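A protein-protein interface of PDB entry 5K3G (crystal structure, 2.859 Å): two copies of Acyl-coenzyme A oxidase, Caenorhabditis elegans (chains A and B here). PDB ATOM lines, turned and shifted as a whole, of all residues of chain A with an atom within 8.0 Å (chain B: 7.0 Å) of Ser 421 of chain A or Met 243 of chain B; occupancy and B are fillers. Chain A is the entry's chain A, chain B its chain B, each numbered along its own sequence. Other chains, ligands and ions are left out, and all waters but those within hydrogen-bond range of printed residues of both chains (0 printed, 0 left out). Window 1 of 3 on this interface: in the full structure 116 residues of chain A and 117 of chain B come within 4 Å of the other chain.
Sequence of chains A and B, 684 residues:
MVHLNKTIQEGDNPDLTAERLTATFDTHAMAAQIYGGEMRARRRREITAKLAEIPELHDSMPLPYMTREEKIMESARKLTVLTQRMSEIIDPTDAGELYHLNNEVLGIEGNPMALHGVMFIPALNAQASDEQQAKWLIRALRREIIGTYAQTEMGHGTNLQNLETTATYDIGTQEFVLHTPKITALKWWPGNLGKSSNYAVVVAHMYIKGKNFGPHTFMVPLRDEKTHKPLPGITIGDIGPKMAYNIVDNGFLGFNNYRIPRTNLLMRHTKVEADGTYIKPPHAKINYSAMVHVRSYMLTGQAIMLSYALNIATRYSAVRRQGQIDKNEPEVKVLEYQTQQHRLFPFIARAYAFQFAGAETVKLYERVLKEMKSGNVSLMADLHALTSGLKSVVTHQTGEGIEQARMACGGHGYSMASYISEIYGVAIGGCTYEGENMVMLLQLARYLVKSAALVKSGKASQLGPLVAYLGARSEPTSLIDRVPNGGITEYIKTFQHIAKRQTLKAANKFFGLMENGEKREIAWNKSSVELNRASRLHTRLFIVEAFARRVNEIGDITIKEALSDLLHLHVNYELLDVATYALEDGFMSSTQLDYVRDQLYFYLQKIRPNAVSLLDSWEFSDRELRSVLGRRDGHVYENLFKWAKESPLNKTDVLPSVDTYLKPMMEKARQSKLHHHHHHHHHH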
ATOM      1  N   ILE A 108     -14.385 -31.546  19.553  1.00  0.00           N
ATOM      2  CA  ILE A 108     -15.048 -30.823  18.475  1.00  0.00           C
ATOM      3  C   ILE A 108     -14.116 -30.489  17.324  1.00  0.00           C
ATOM      4  O   ILE A 108     -14.575 -29.942  16.312  1.00  0.00           O
ATOM      5  CB  ILE A 108     -15.696 -29.527  19.002  1.00  0.00           C
ATOM      6  CG1 ILE A 108     -14.645 -28.638  19.673  1.00  0.00           C
ATOM      7  CG2 ILE A 108     -16.827 -29.858  19.965  1.00  0.00           C
ATOM      8  CD1 ILE A 108     -15.164 -27.272  20.067  1.00  0.00           C
ATOM      9  N   MET A 243      -9.221 -22.049  10.095  1.00  0.00           N
ATOM     10  CA  MET A 243      -9.441 -21.250  11.295  1.00  0.00           C
ATOM     11  C   MET A 243      -9.763 -22.117  12.496  1.00  0.00           C
ATOM     12  O   MET A 243      -9.576 -21.675  13.633  1.00  0.00           O
ATOM     13  CB  MET A 243     -10.561 -20.231  11.077  1.00  0.00           C
ATOM     14  CG  MET A 243     -11.967 -20.802  11.020  1.00  0.00           C
ATOM     15  SD  MET A 243     -13.206 -19.529  10.678  1.00  0.00           S
ATOM     16  CE  MET A 243     -13.350 -18.735  12.283  1.00  0.00           C
ATOM     17  N   ALA A 244     -10.223 -23.341  12.268  1.00  0.00           N
ATOM     18  CA  ALA A 244     -10.569 -24.288  13.320  1.00  0.00           C
ATOM     19  C   ALA A 244     -10.784 -25.647  12.666  1.00  0.00           C
ATOM     20  O   ALA A 244     -10.630 -25.804  11.450  1.00  0.00           O
ATOM     21  CB  ALA A 244     -11.808 -23.832  14.089  1.00  0.00           C
ATOM     22  N   ALA A 309     -20.571 -22.897  25.265  1.00  0.00           N
ATOM     23  CA  ALA A 309     -20.006 -21.574  25.503  1.00  0.00           C
ATOM     24  C   ALA A 309     -20.705 -20.864  26.652  1.00  0.00           C
ATOM     25  O   ALA A 309     -20.063 -20.145  27.425  1.00  0.00           O
ATOM     26  CB  ALA A 309     -20.088 -20.744  24.223  1.00  0.00           C
ATOM     27  N   ILE A 312     -19.575 -22.110  29.954  1.00  0.00           N
ATOM     28  CA  ILE A 312     -18.278 -21.534  30.285  1.00  0.00           C
ATOM     29  C   ILE A 312     -18.438 -20.105  30.783  1.00  0.00           C
ATOM     30  O   ILE A 312     -17.892 -19.733  31.828  1.00  0.00           O
ATOM     31  CB  ILE A 312     -17.344 -21.610  29.064  1.00  0.00           C
ATOM     32  CG1 ILE A 312     -17.126 -23.075  28.668  1.00  0.00           C
ATOM     33  CG2 ILE A 312     -16.022 -20.905  29.357  1.00  0.00           C
ATOM     34  CD1 ILE A 312     -16.561 -23.261  27.286  1.00  0.00           C
ATOM     35  N   ILE A 402     -22.314 -17.378  20.853  1.00  0.00           N
ATOM     36  CA  ILE A 402     -21.020 -17.902  21.275  1.00  0.00           C
ATOM     37  C   ILE A 402     -20.007 -16.772  21.431  1.00  0.00           C
ATOM     38  O   ILE A 402     -19.278 -16.701  22.428  1.00  0.00           O
ATOM     39  CB  ILE A 402     -20.529 -18.968  20.281  1.00  0.00           C
ATOM     40  CG1 ILE A 402     -21.317 -20.271  20.446  1.00  0.00           C
ATOM     41  CG2 ILE A 402     -19.039 -19.198  20.462  1.00  0.00           C
ATOM     42  CD1 ILE A 402     -21.055 -21.250  19.328  1.00  0.00           C
ATOM     43  N   GLU A 403     -19.947 -15.874  20.445  1.00  0.00           N
ATOM     44  CA  GLU A 403     -19.053 -14.724  20.525  1.00  0.00           C
ATOM     45  C   GLU A 403     -19.476 -13.771  21.631  1.00  0.00           C
ATOM     46  O   GLU A 403     -18.622 -13.168  22.292  1.00  0.00           O
ATOM     47  CB  GLU A 403     -19.014 -14.000  19.181  1.00  0.00           C
ATOM     48  CG  GLU A 403     -17.891 -12.981  19.040  1.00  0.00           C
ATOM     49  CD  GLU A 403     -16.513 -13.615  19.097  1.00  0.00           C
ATOM     50  OE1 GLU A 403     -16.349 -14.737  18.571  1.00  0.00           O
ATOM     51  OE2 GLU A 403     -15.592 -12.990  19.666  1.00  0.00           O
ATOM     52  N   ARG A 406     -18.031 -15.344  24.682  1.00  0.00           N
ATOM     53  CA  ARG A 406     -16.598 -15.125  24.856  1.00  0.00           C
ATOM     54  C   ARG A 406     -16.326 -13.745  25.445  1.00  0.00           C
ATOM     55  O   ARG A 406     -15.511 -13.601  26.363  1.00  0.00           O
ATOM     56  CB  ARG A 406     -15.861 -15.307  23.527  1.00  0.00           C
ATOM     57  CG  ARG A 406     -14.357 -15.500  23.700  1.00  0.00           C
ATOM     58  CD  ARG A 406     -13.605 -15.391  22.377  1.00  0.00           C
ATOM     59  NE  ARG A 406     -13.951 -14.183  21.627  1.00  0.00           N
ATOM     60  CZ  ARG A 406     -13.568 -12.950  21.951  1.00  0.00           C
ATOM     61  NH1 ARG A 406     -12.833 -12.739  23.031  1.00  0.00           N
ATOM     62  NH2 ARG A 406     -13.934 -11.920  21.198  1.00  0.00           N
ATOM     63  N   GLY A 411     -11.149 -10.300  29.260  1.00  0.00           N
ATOM     64  CA  GLY A 411      -9.859 -10.629  28.672  1.00  0.00           C
ATOM     65  C   GLY A 411      -9.540 -12.109  28.734  1.00  0.00           C
ATOM     66  O   GLY A 411      -8.952 -12.666  27.804  1.00  0.00           O
ATOM     67  N   GLY A 413     -11.418 -14.521  28.310  1.00  0.00           N
ATOM     68  CA  GLY A 413     -12.042 -15.225  27.202  1.00  0.00           C
ATOM     69  C   GLY A 413     -11.157 -15.301  25.973  1.00  0.00           C
ATOM     70  O   GLY A 413     -11.333 -16.183  25.129  1.00  0.00           O
ATOM     71  N   TYR A 414     -10.186 -14.393  25.862  1.00  0.00           N
ATOM     72  CA  TYR A 414      -9.277 -14.406  24.720  1.00  0.00           C
ATOM     73  C   TYR A 414      -8.324 -15.597  24.772  1.00  0.00           C
ATOM     74  O   TYR A 414      -7.815 -16.031  23.732  1.00  0.00           O
ATOM     75  CB  TYR A 414      -8.512 -13.083  24.683  1.00  0.00           C
ATOM     76  CG  TYR A 414      -7.856 -12.723  23.370  1.00  0.00           C
ATOM     77  CD1 TYR A 414      -8.579 -12.109  22.351  1.00  0.00           C
ATOM     78  CD2 TYR A 414      -6.504 -12.955  23.161  1.00  0.00           C
ATOM     79  CE1 TYR A 414      -7.975 -11.761  21.152  1.00  0.00           C
ATOM     80  CE2 TYR A 414      -5.890 -12.608  21.971  1.00  0.00           C
ATOM     81  CZ  TYR A 414      -6.631 -12.012  20.968  1.00  0.00           C
ATOM     82  OH  TYR A 414      -6.032 -11.663  19.779  1.00  0.00           O
ATOM     83  N   SER A 415      -8.064 -16.132  25.962  1.00  0.00           N
ATOM     84  CA  SER A 415      -7.171 -17.275  26.090  1.00  0.00           C
ATOM     85  C   SER A 415      -7.831 -18.520  25.517  1.00  0.00           C
ATOM     86  O   SER A 415      -9.058 -18.646  25.499  1.00  0.00           O
ATOM     87  CB  SER A 415      -6.801 -17.497  27.562  1.00  0.00           C
ATOM     88  OG  SER A 415      -6.017 -18.666  27.750  1.00  0.00           O
ATOM     89  N   MET A 416      -7.002 -19.449  25.034  1.00  0.00           N
ATOM     90  CA  MET A 416      -7.507 -20.790  24.761  1.00  0.00           C
ATOM     91  C   MET A 416      -7.958 -21.495  26.031  1.00  0.00           C
ATOM     92  O   MET A 416      -8.578 -22.561  25.947  1.00  0.00           O
ATOM     93  CB  MET A 416      -6.442 -21.627  24.053  1.00  0.00           C
ATOM     94  CG  MET A 416      -6.061 -21.116  22.675  1.00  0.00           C
ATOM     95  SD  MET A 416      -7.475 -20.853  21.581  1.00  0.00           S
ATOM     96  CE  MET A 416      -8.257 -22.467  21.592  1.00  0.00           C
ATOM     97  N   ALA A 417      -7.664 -20.922  27.201  1.00  0.00           N
ATOM     98  CA  ALA A 417      -8.153 -21.487  28.451  1.00  0.00           C
ATOM     99  C   ALA A 417      -9.665 -21.351  28.571  1.00  0.00           C
ATOM    100  O   ALA A 417     -10.296 -22.118  29.302  1.00  0.00           O
ATOM    101  CB  ALA A 417      -7.463 -20.819  29.636  1.00  0.00           C
ATOM    102  N   SER A 418     -10.261 -20.382  27.874  1.00  0.00           N
ATOM    103  CA  SER A 418     -11.717 -20.325  27.797  1.00  0.00           C
ATOM    104  C   SER A 418     -12.250 -21.376  26.831  1.00  0.00           C
ATOM    105  O   SER A 418     -13.292 -21.988  27.095  1.00  0.00           O
ATOM    106  CB  SER A 418     -12.176 -18.935  27.372  1.00  0.00           C
ATOM    107  OG  SER A 418     -12.293 -18.860  25.957  1.00  0.00           O
ATOM    108  N   TYR A 419     -11.546 -21.584  25.714  1.00  0.00           N
ATOM    109  CA  TYR A 419     -11.843 -22.530  24.644  1.00  0.00           C
ATOM    110  C   TYR A 419     -13.017 -22.080  23.791  1.00  0.00           C
ATOM    111  O   TYR A 419     -13.363 -22.771  22.826  1.00  0.00           O
ATOM    112  CB  TYR A 419     -12.109 -23.947  25.177  1.00  0.00           C
ATOM    113  CG  TYR A 419     -11.888 -25.053  24.165  1.00  0.00           C
ATOM    114  CD1 TYR A 419     -10.632 -25.273  23.620  1.00  0.00           C
ATOM    115  CD2 TYR A 419     -12.934 -25.878  23.760  1.00  0.00           C
ATOM    116  CE1 TYR A 419     -10.417 -26.274  22.695  1.00  0.00           C
ATOM    117  CE2 TYR A 419     -12.724 -26.892  22.831  1.00  0.00           C
ATOM    118  CZ  TYR A 419     -11.459 -27.086  22.304  1.00  0.00           C
ATOM    119  OH  TYR A 419     -11.219 -28.079  21.374  1.00  0.00           O
ATOM    120  N   ILE A 420     -13.627 -20.929  24.092  1.00  0.00           N
ATOM    121  CA  ILE A 420     -14.821 -20.492  23.370  1.00  0.00           C
ATOM    122  C   ILE A 420     -14.486 -20.144  21.928  1.00  0.00           C
ATOM    123  O   ILE A 420     -15.330 -20.281  21.033  1.00  0.00           O
ATOM    124  CB  ILE A 420     -15.471 -19.305  24.109  1.00  0.00           C
ATOM    125  CG1 ILE A 420     -15.908 -19.745  25.506  1.00  0.00           C
ATOM    126  CG2 ILE A 420     -16.645 -18.759  23.333  1.00  0.00           C
ATOM    127  CD1 ILE A 420     -16.330 -18.606  26.400  1.00  0.00           C
ATOM    128  N   SER A 421     -13.251 -19.713  21.669  1.00  0.00           N
ATOM    129  CA  SER A 421     -12.874 -19.347  20.310  1.00  0.00           C
ATOM    130  C   SER A 421     -12.909 -20.556  19.381  1.00  0.00           C
ATOM    131  O   SER A 421     -13.370 -20.450  18.240  1.00  0.00           O
ATOM    132  CB  SER A 421     -11.491 -18.702  20.306  1.00  0.00           C
ATOM    133  OG  SER A 421     -10.475 -19.689  20.392  1.00  0.00           O
ATOM    134  N   GLU A 422     -12.440 -21.716  19.856  1.00  0.00           N
ATOM    135  CA  GLU A 422     -12.497 -22.929  19.047  1.00  0.00           C
ATOM    136  C   GLU A 422     -13.926 -23.435  18.917  1.00  0.00           C
ATOM    137  O   GLU A 422     -14.290 -23.998  17.879  1.00  0.00           O
ATOM    138  CB  GLU A 422     -11.601 -24.012  19.650  1.00  0.00           C
ATOM    139  CG  GLU A 422     -11.440 -25.269  18.788  1.00  0.00           C
ATOM    140  CD  GLU A 422     -10.682 -25.014  17.504  1.00  0.00           C
ATOM    141  OE1 GLU A 422      -9.894 -24.046  17.456  1.00  0.00           O
ATOM    142  OE2 GLU A 422     -10.883 -25.784  16.544  1.00  0.00           O
ATOM    143  N   ILE A 423     -14.740 -23.256  19.960  1.00  0.00           N
ATOM    144  CA  ILE A 423     -16.163 -23.577  19.862  1.00  0.00           C
ATOM    145  C   ILE A 423     -16.820 -22.741  18.774  1.00  0.00           C
ATOM    146  O   ILE A 423     -17.584 -23.251  17.945  1.00  0.00           O
ATOM    147  CB  ILE A 423     -16.854 -23.373  21.220  1.00  0.00           C
ATOM    148  CG1 ILE A 423     -16.355 -24.412  22.223  1.00  0.00           C
ATOM    149  CG2 ILE A 423     -18.366 -23.435  21.063  1.00  0.00           C
ATOM    150  CD1 ILE A 423     -16.598 -24.027  23.654  1.00  0.00           C
ATOM    151  N   TYR A 424     -16.531 -21.438  18.762  1.00  0.00           N
ATOM    152  CA  TYR A 424     -17.051 -20.570  17.712  1.00  0.00           C
ATOM    153  C   TYR A 424     -16.650 -21.073  16.333  1.00  0.00           C
ATOM    154  O   TYR A 424     -17.487 -21.196  15.430  1.00  0.00           O
ATOM    155  CB  TYR A 424     -16.543 -19.144  17.919  1.00  0.00           C
ATOM    156  CG  TYR A 424     -17.010 -18.206  16.840  1.00  0.00           C
ATOM    157  CD1 TYR A 424     -18.280 -17.655  16.889  1.00  0.00           C
ATOM    158  CD2 TYR A 424     -16.189 -17.871  15.770  1.00  0.00           C
ATOM    159  CE1 TYR A 424     -18.721 -16.791  15.916  1.00  0.00           C
ATOM    160  CE2 TYR A 424     -16.626 -17.006  14.780  1.00  0.00           C
ATOM    161  CZ  TYR A 424     -17.895 -16.468  14.867  1.00  0.00           C
ATOM    162  OH  TYR A 424     -18.369 -15.618  13.902  1.00  0.00           O
ATOM    163  N   GLY A 425     -15.363 -21.374  16.159  1.00  0.00           N
ATOM    164  CA  GLY A 425     -14.857 -21.715  14.840  1.00  0.00           C
ATOM    165  C   GLY A 425     -15.450 -22.989  14.276  1.00  0.00           C
ATOM    166  O   GLY A 425     -15.676 -23.094  13.068  1.00  0.00           O
ATOM    167  N   VAL A 426     -15.717 -23.974  15.137  1.00  0.00           N
ATOM    168  CA  VAL A 426     -16.314 -25.214  14.651  1.00  0.00           C
ATOM    169  C   VAL A 426     -17.795 -25.011  14.365  1.00  0.00           C
ATOM    170  O   VAL A 426     -18.319 -25.483  13.347  1.00  0.00           O
ATOM    171  CB  VAL A 426     -16.083 -26.357  15.655  1.00  0.00           C
ATOM    172  CG1 VAL A 426     -16.725 -27.641  15.145  1.00  0.00           C
ATOM    173  CG2 VAL A 426     -14.601 -26.557  15.890  1.00  0.00           C
ATOM    174  N   ALA A 427     -18.483 -24.284  15.247  1.00  0.00           N
ATOM    175  CA  ALA A 427     -19.919 -24.094  15.097  1.00  0.00           C
ATOM    176  C   ALA A 427     -20.249 -23.294  13.842  1.00  0.00           C
ATOM    177  O   ALA A 427     -21.226 -23.597  13.152  1.00  0.00           O
ATOM    178  CB  ALA A 427     -20.483 -23.413  16.339  1.00  0.00           C
ATOM    179  N   ILE A 428     -19.443 -22.277  13.522  1.00  0.00           N
ATOM    180  CA  ILE A 428     -19.752 -21.404  12.393  1.00  0.00           C
ATOM    181  C   ILE A 428     -19.514 -22.101  11.059  1.00  0.00           C
ATOM    182  O   ILE A 428     -20.049 -21.669  10.030  1.00  0.00           O
ATOM    183  CB  ILE A 428     -18.929 -20.103  12.502  1.00  0.00           C
ATOM    184  CG1 ILE A 428     -19.694 -18.921  11.904  1.00  0.00           C
ATOM    185  CG2 ILE A 428     -17.569 -20.266  11.846  1.00  0.00           C
ATOM    186  CD1 ILE A 428     -20.875 -18.466  12.742  1.00  0.00           C
ATOM    187  N   PRO B 241      -1.286 -20.294  25.092  1.00  0.00           N
ATOM    188  CA  PRO B 241      -1.739 -19.889  23.759  1.00  0.00           C
ATOM    189  C   PRO B 241      -3.082 -19.181  23.817  1.00  0.00           C
ATOM    190  O   PRO B 241      -3.872 -19.367  24.745  1.00  0.00           O
ATOM    191  CB  PRO B 241      -1.844 -21.215  23.004  1.00  0.00           C
ATOM    192  CG  PRO B 241      -2.154 -22.210  24.072  1.00  0.00           C
ATOM    193  CD  PRO B 241      -1.403 -21.745  25.298  1.00  0.00           C
ATOM    194  N   LYS B 242      -3.330 -18.346  22.808  1.00  0.00           N
ATOM    195  CA  LYS B 242      -4.529 -17.521  22.748  1.00  0.00           C
ATOM    196  C   LYS B 242      -5.241 -17.769  21.424  1.00  0.00           C
ATOM    197  O   LYS B 242      -4.744 -18.488  20.552  1.00  0.00           O
ATOM    198  CB  LYS B 242      -4.184 -16.036  22.919  1.00  0.00           C
ATOM    199  CG  LYS B 242      -3.341 -15.730  24.154  1.00  0.00           C
ATOM    200  CD  LYS B 242      -2.557 -14.440  23.992  1.00  0.00           C
ATOM    201  CE  LYS B 242      -1.544 -14.534  22.861  1.00  0.00           C
ATOM    202  NZ  LYS B 242      -0.675 -13.328  22.806  1.00  0.00           N
ATOM    203  N   MET B 243      -6.425 -17.166  21.269  1.00  0.00           N
ATOM    204  CA  MET B 243      -7.184 -17.360  20.039  1.00  0.00           C
ATOM    205  C   MET B 243      -6.490 -16.731  18.846  1.00  0.00           C
ATOM    206  O   MET B 243      -6.740 -17.142  17.709  1.00  0.00           O
ATOM    207  CB  MET B 243      -8.602 -16.795  20.171  1.00  0.00           C
ATOM    208  CG  MET B 243      -8.701 -15.285  20.219  1.00  0.00           C
ATOM    209  SD  MET B 243     -10.401 -14.710  20.437  1.00  0.00           S
ATOM    210  CE  MET B 243     -11.079 -14.980  18.797  1.00  0.00           C
ATOM    211  N   ALA B 244      -5.612 -15.767  19.086  1.00  0.00           N
ATOM    212  CA  ALA B 244      -4.844 -15.103  18.038  1.00  0.00           C
ATOM    213  C   ALA B 244      -3.743 -14.295  18.708  1.00  0.00           C
ATOM    214  O   ALA B 244      -3.588 -14.321  19.933  1.00  0.00           O
ATOM    215  CB  ALA B 244      -5.740 -14.214  17.169  1.00  0.00           C
ATOM    216  N   TYR B 245      -2.981 -13.566  17.885  1.00  0.00           N
ATOM    217  CA  TYR B 245      -1.922 -12.668  18.363  1.00  0.00           C
ATOM    218  C   TYR B 245      -0.848 -13.440  19.127  1.00  0.00           C
ATOM    219  O   TYR B 245      -0.325 -12.973  20.141  1.00  0.00           O
ATOM    220  CB  TYR B 245      -2.511 -11.548  19.235  1.00  0.00           C
ATOM    221  CG  TYR B 245      -1.707 -10.266  19.331  1.00  0.00           C
ATOM    222  CD1 TYR B 245      -1.336  -9.560  18.190  1.00  0.00           C
ATOM    223  CD2 TYR B 245      -1.382  -9.727  20.566  1.00  0.00           C
ATOM    224  CE1 TYR B 245      -0.629  -8.375  18.284  1.00  0.00           C
ATOM    225  CE2 TYR B 245      -0.681  -8.544  20.670  1.00  0.00           C
ATOM    226  CZ  TYR B 245      -0.303  -7.873  19.525  1.00  0.00           C
ATOM    227  OH  TYR B 245       0.389  -6.688  19.622  1.00  0.00           O
ATOM    228  N   ASN B 246      -0.507 -14.628  18.635  1.00  0.00           N
ATOM    229  CA  ASN B 246       0.257 -15.565  19.444  1.00  0.00           C
ATOM    230  C   ASN B 246       1.762 -15.368  19.330  1.00  0.00           C
ATOM    231  O   ASN B 246       2.509 -16.127  19.953  1.00  0.00           O
ATOM    232  CB  ASN B 246      -0.110 -17.007  19.072  1.00  0.00           C
ATOM    233  CG  ASN B 246      -1.342 -17.515  19.804  1.00  0.00           C
ATOM    234  OD1 ASN B 246      -1.322 -17.700  21.023  1.00  0.00           O
ATOM    235  ND2 ASN B 246      -2.409 -17.772  19.056  1.00  0.00           N
ATOM    236  N   SER B 421      -9.712 -14.933   9.481  1.00  0.00           N
ATOM    237  CA  SER B 421      -9.923 -15.389  10.852  1.00  0.00           C
ATOM    238  C   SER B 421      -8.878 -14.808  11.795  1.00  0.00           C
ATOM    239  O   SER B 421      -9.201 -14.436  12.929  1.00  0.00           O
ATOM    240  CB  SER B 421      -9.907 -16.914  10.912  1.00  0.00           C
ATOM    241  OG  SER B 421      -8.583 -17.413  10.872  1.00  0.00           O
ATOM    242  N   GLU B 422      -7.622 -14.717  11.347  1.00  0.00           N
ATOM    243  CA  GLU B 422      -6.583 -14.124  12.182  1.00  0.00           C
ATOM    244  C   GLU B 422      -6.746 -12.615  12.269  1.00  0.00           C
ATOM    245  O   GLU B 422      -6.468 -12.016  13.313  1.00  0.00           O
ATOM    246  CB  GLU B 422      -5.198 -14.487  11.643  1.00  0.00           C
ATOM    247  CG  GLU B 422      -4.033 -14.061  12.542  1.00  0.00           C
ATOM    248  CD  GLU B 422      -4.003 -14.812  13.854  1.00  0.00           C
ATOM    249  OE1 GLU B 422      -4.531 -15.943  13.904  1.00  0.00           O
ATOM    250  OE2 GLU B 422      -3.452 -14.268  14.832  1.00  0.00           O
ATOM    251  N   TYR B 424      -9.659 -11.124  12.228  1.00  0.00           N
ATOM    252  CA  TYR B 424     -10.718 -11.001  13.221  1.00  0.00           C
ATOM    253  C   TYR B 424     -10.162 -11.102  14.636  1.00  0.00           C
ATOM    254  O   TYR B 424     -10.440 -10.256  15.495  1.00  0.00           O
ATOM    255  CB  TYR B 424     -11.773 -12.083  12.993  1.00  0.00           C
ATOM    256  CG  TYR B 424     -12.878 -12.049  14.007  1.00  0.00           C
ATOM    257  CD1 TYR B 424     -13.892 -11.108  13.913  1.00  0.00           C
ATOM    258  CD2 TYR B 424     -12.908 -12.948  15.063  1.00  0.00           C
ATOM    259  CE1 TYR B 424     -14.907 -11.064  14.839  1.00  0.00           C
ATOM    260  CE2 TYR B 424     -13.922 -12.908  16.001  1.00  0.00           C
ATOM    261  CZ  TYR B 424     -14.920 -11.961  15.877  1.00  0.00           C
ATOM    262  OH  TYR B 424     -15.947 -11.899  16.781  1.00  0.00           O
ATOM    263  N   GLY B 425      -9.351 -12.131  14.887  1.00  0.00           N
ATOM    264  CA  GLY B 425      -8.903 -12.400  16.244  1.00  0.00           C
ATOM    265  C   GLY B 425      -8.028 -11.301  16.814  1.00  0.00           C
ATOM    266  O   GLY B 425      -8.091 -11.006  18.009  1.00  0.00           O
ATOM    267  N   VAL B 426      -7.205 -10.675  15.968  1.00  0.00           N
ATOM    268  CA  VAL B 426      -6.358  -9.591  16.451  1.00  0.00           C
ATOM    269  C   VAL B 426      -7.176  -8.327  16.667  1.00  0.00           C
ATOM    270  O   VAL B 426      -7.024  -7.638  17.684  1.00  0.00           O
ATOM    271  CB  VAL B 426      -5.184  -9.347  15.490  1.00  0.00           C
ATOM    272  CG1 VAL B 426      -4.319  -8.206  16.000  1.00  0.00           C
ATOM    273  CG2 VAL B 426      -4.358 -10.609  15.336  1.00  0.00           C
ATOM    274  N   ILE B 428     -10.274  -7.963  17.458  1.00  0.00           N
ATOM    275  CA  ILE B 428     -11.270  -8.025  18.521  1.00  0.00           C
ATOM    276  C   ILE B 428     -10.641  -7.911  19.906  1.00  0.00           C
ATOM    277  O   ILE B 428     -11.353  -7.647  20.882  1.00  0.00           O
ATOM    278  CB  ILE B 428     -12.093  -9.324  18.392  1.00  0.00           C
ATOM    279  CG1 ILE B 428     -13.507  -9.130  18.947  1.00  0.00           C
ATOM    280  CG2 ILE B 428     -11.378 -10.485  19.082  1.00  0.00           C
ATOM    281  CD1 ILE B 428     -14.410  -8.336  18.024  1.00  0.00           C
ATOM    282  N   GLY B 429      -9.327  -8.085  20.020  1.00  0.00           N
ATOM    283  CA  GLY B 429      -8.651  -8.123  21.311  1.00  0.00           C
ATOM    284  C   GLY B 429      -8.172  -6.789  21.855  1.00  0.00           C
ATOM    285  O   GLY B 429      -8.581  -5.729  21.380  1.00  0.00           O
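The side-chain carboxylate (OE2) of Glu 403 of chain A is in salt-bridge range of the guanidinium group (NH2) of Arg 406 of chain A, 2.5 Å away.
The side-chain hydroxyl (OG) of Ser 418 of chain A is in hydrogen-bond range of the backbone carbonyl oxygen (O) of Ser 415 of chain A (3.3 Å).
The side-chain sulfur (SD) of Met 416 of chain A sits at hydrogen-bond distance from the side-chain hydroxyl (OG) of Ser 421 of chain A (3.4 Å).
The side-chain amino group (NZ) of Lys 242 of chain B lies within hydrogen-bond range of the backbone carbonyl oxygen (O) of Tyr 245 of chain B (2.7 Å).
N of Lys 242 of chain B sits at hydrogen-bond distance from OD1 of Asn 246 of chain B (2.8 Å).
The backbone NH of Tyr 245 of chain B sits at hydrogen-bond distance from the side-chain carboxylate of Glu 422 of chain B.
Among the printed residues, merely in contact across the chains: Met 243 of chain A with Ser 421 of chain B (3.4 Å), Ser 421 of chain A with Met 243 of chain B (3.5 Å), Tyr 414 of chain A with Ala 244 of chain B (3.5 Å), Tyr 414 of chain A with Tyr 245 of chain B (3.6 Å), Arg 406 of chain A with Ile 428 of chain B (3.6 Å), Tyr 414 of chain A with Gly 429 of chain B (3.7 Å), Tyr 414 of chain A with Lys 242 of chain B (3.7 Å), Ser 415 of chain A with Pro 241 of chain B (3.8 Å), Met 416 of chain A with Met 243 of chain B (3.8 Å) and Tyr 414 of chain A with Val 426 of chain B (3.9 Å).
Of the 25 printed residues of chain A, 7 touch a printed residue of chain B.
Hydrophobic or aromatic side chains of chain A within 4 Å of the printed part of chain B: Met 243, Tyr 414 and Met 416.
Of the 13 printed residues of chain B, 11 touch a printed residue of chain A.
Hydrophobic or aromatic side chains of chain B within 4 Å of the printed part of chain A: Met 243, Ala 244, Tyr 245, Tyr 424 and Ile 428.
Along chain B the printed residues that touch a printed residue of chain A span positions 241 to 429.
Met 243 of chain A touches Ser 421 of chain B, and with the chains exchanged Ser 421 of chain A touches Met 243 of chain B.
OE2 of Glu 403 of chain A sits close to OH of Tyr 424 of chain B, at 3.1 Å.
NE of Arg 406 of chain A sits at hydrogen-bond distance from SD of Met 243 of chain B, at 3.8 Å.
O of Tyr 414 of chain A is in hydrogen-bond range of N of Met 243 of chain B.
OH of Tyr 414 of chain A sits at hydrogen-bond distance from O of Gly 425 of chain B, at 2.8 Å.
The backbone NH of Met 416 of chain A sits at hydrogen-bond distance from the backbone carbonyl oxygen of Pro 241 of chain B (3.1 Å).
The side-chain sulfur (SD) of Met 416 of chain A sits close to the backbone carbonyl oxygen (O) of Lys 242 of chain B, 3.8 Å away.
Ser 421 of chain A touches just one residue of chain B: Met 243 (3.5 Å).
Of chain A, only Arg 406, Tyr 414, Met 416 and Ser 421 come within 4 Å of Met 243 of chain B.
Of chain A, only Tyr 414 (3.5 Å) comes within 4 Å of Ala 244 of chain B.
Printed residues of chain B within 4 Å of Met 243 of chain A: Ser 421.
Of the printed residues of chain A, Ile 428 of chain B touches Arg 406.
Printed residues of chain A within 4 Å of Lys 242 of chain B: Tyr 414 (3.7 Å) and Met 416 (3.6 Å).
Printed residues of chain A within 4 Å of Tyr 424 of chain B: Glu 403.
Val 426 of chain A touches none of the printed residues of chain B.
Tyr 419 of chain A touches none of the printed residues of chain B.
The nearest residue of chain B that does not touch Ser 421 of chain A is Lys 242 of chain B (5.7 Å).
The nearest residue of chain A that does not touch Met 243 of chain B is Ser 415 of chain A (4.7 Å).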
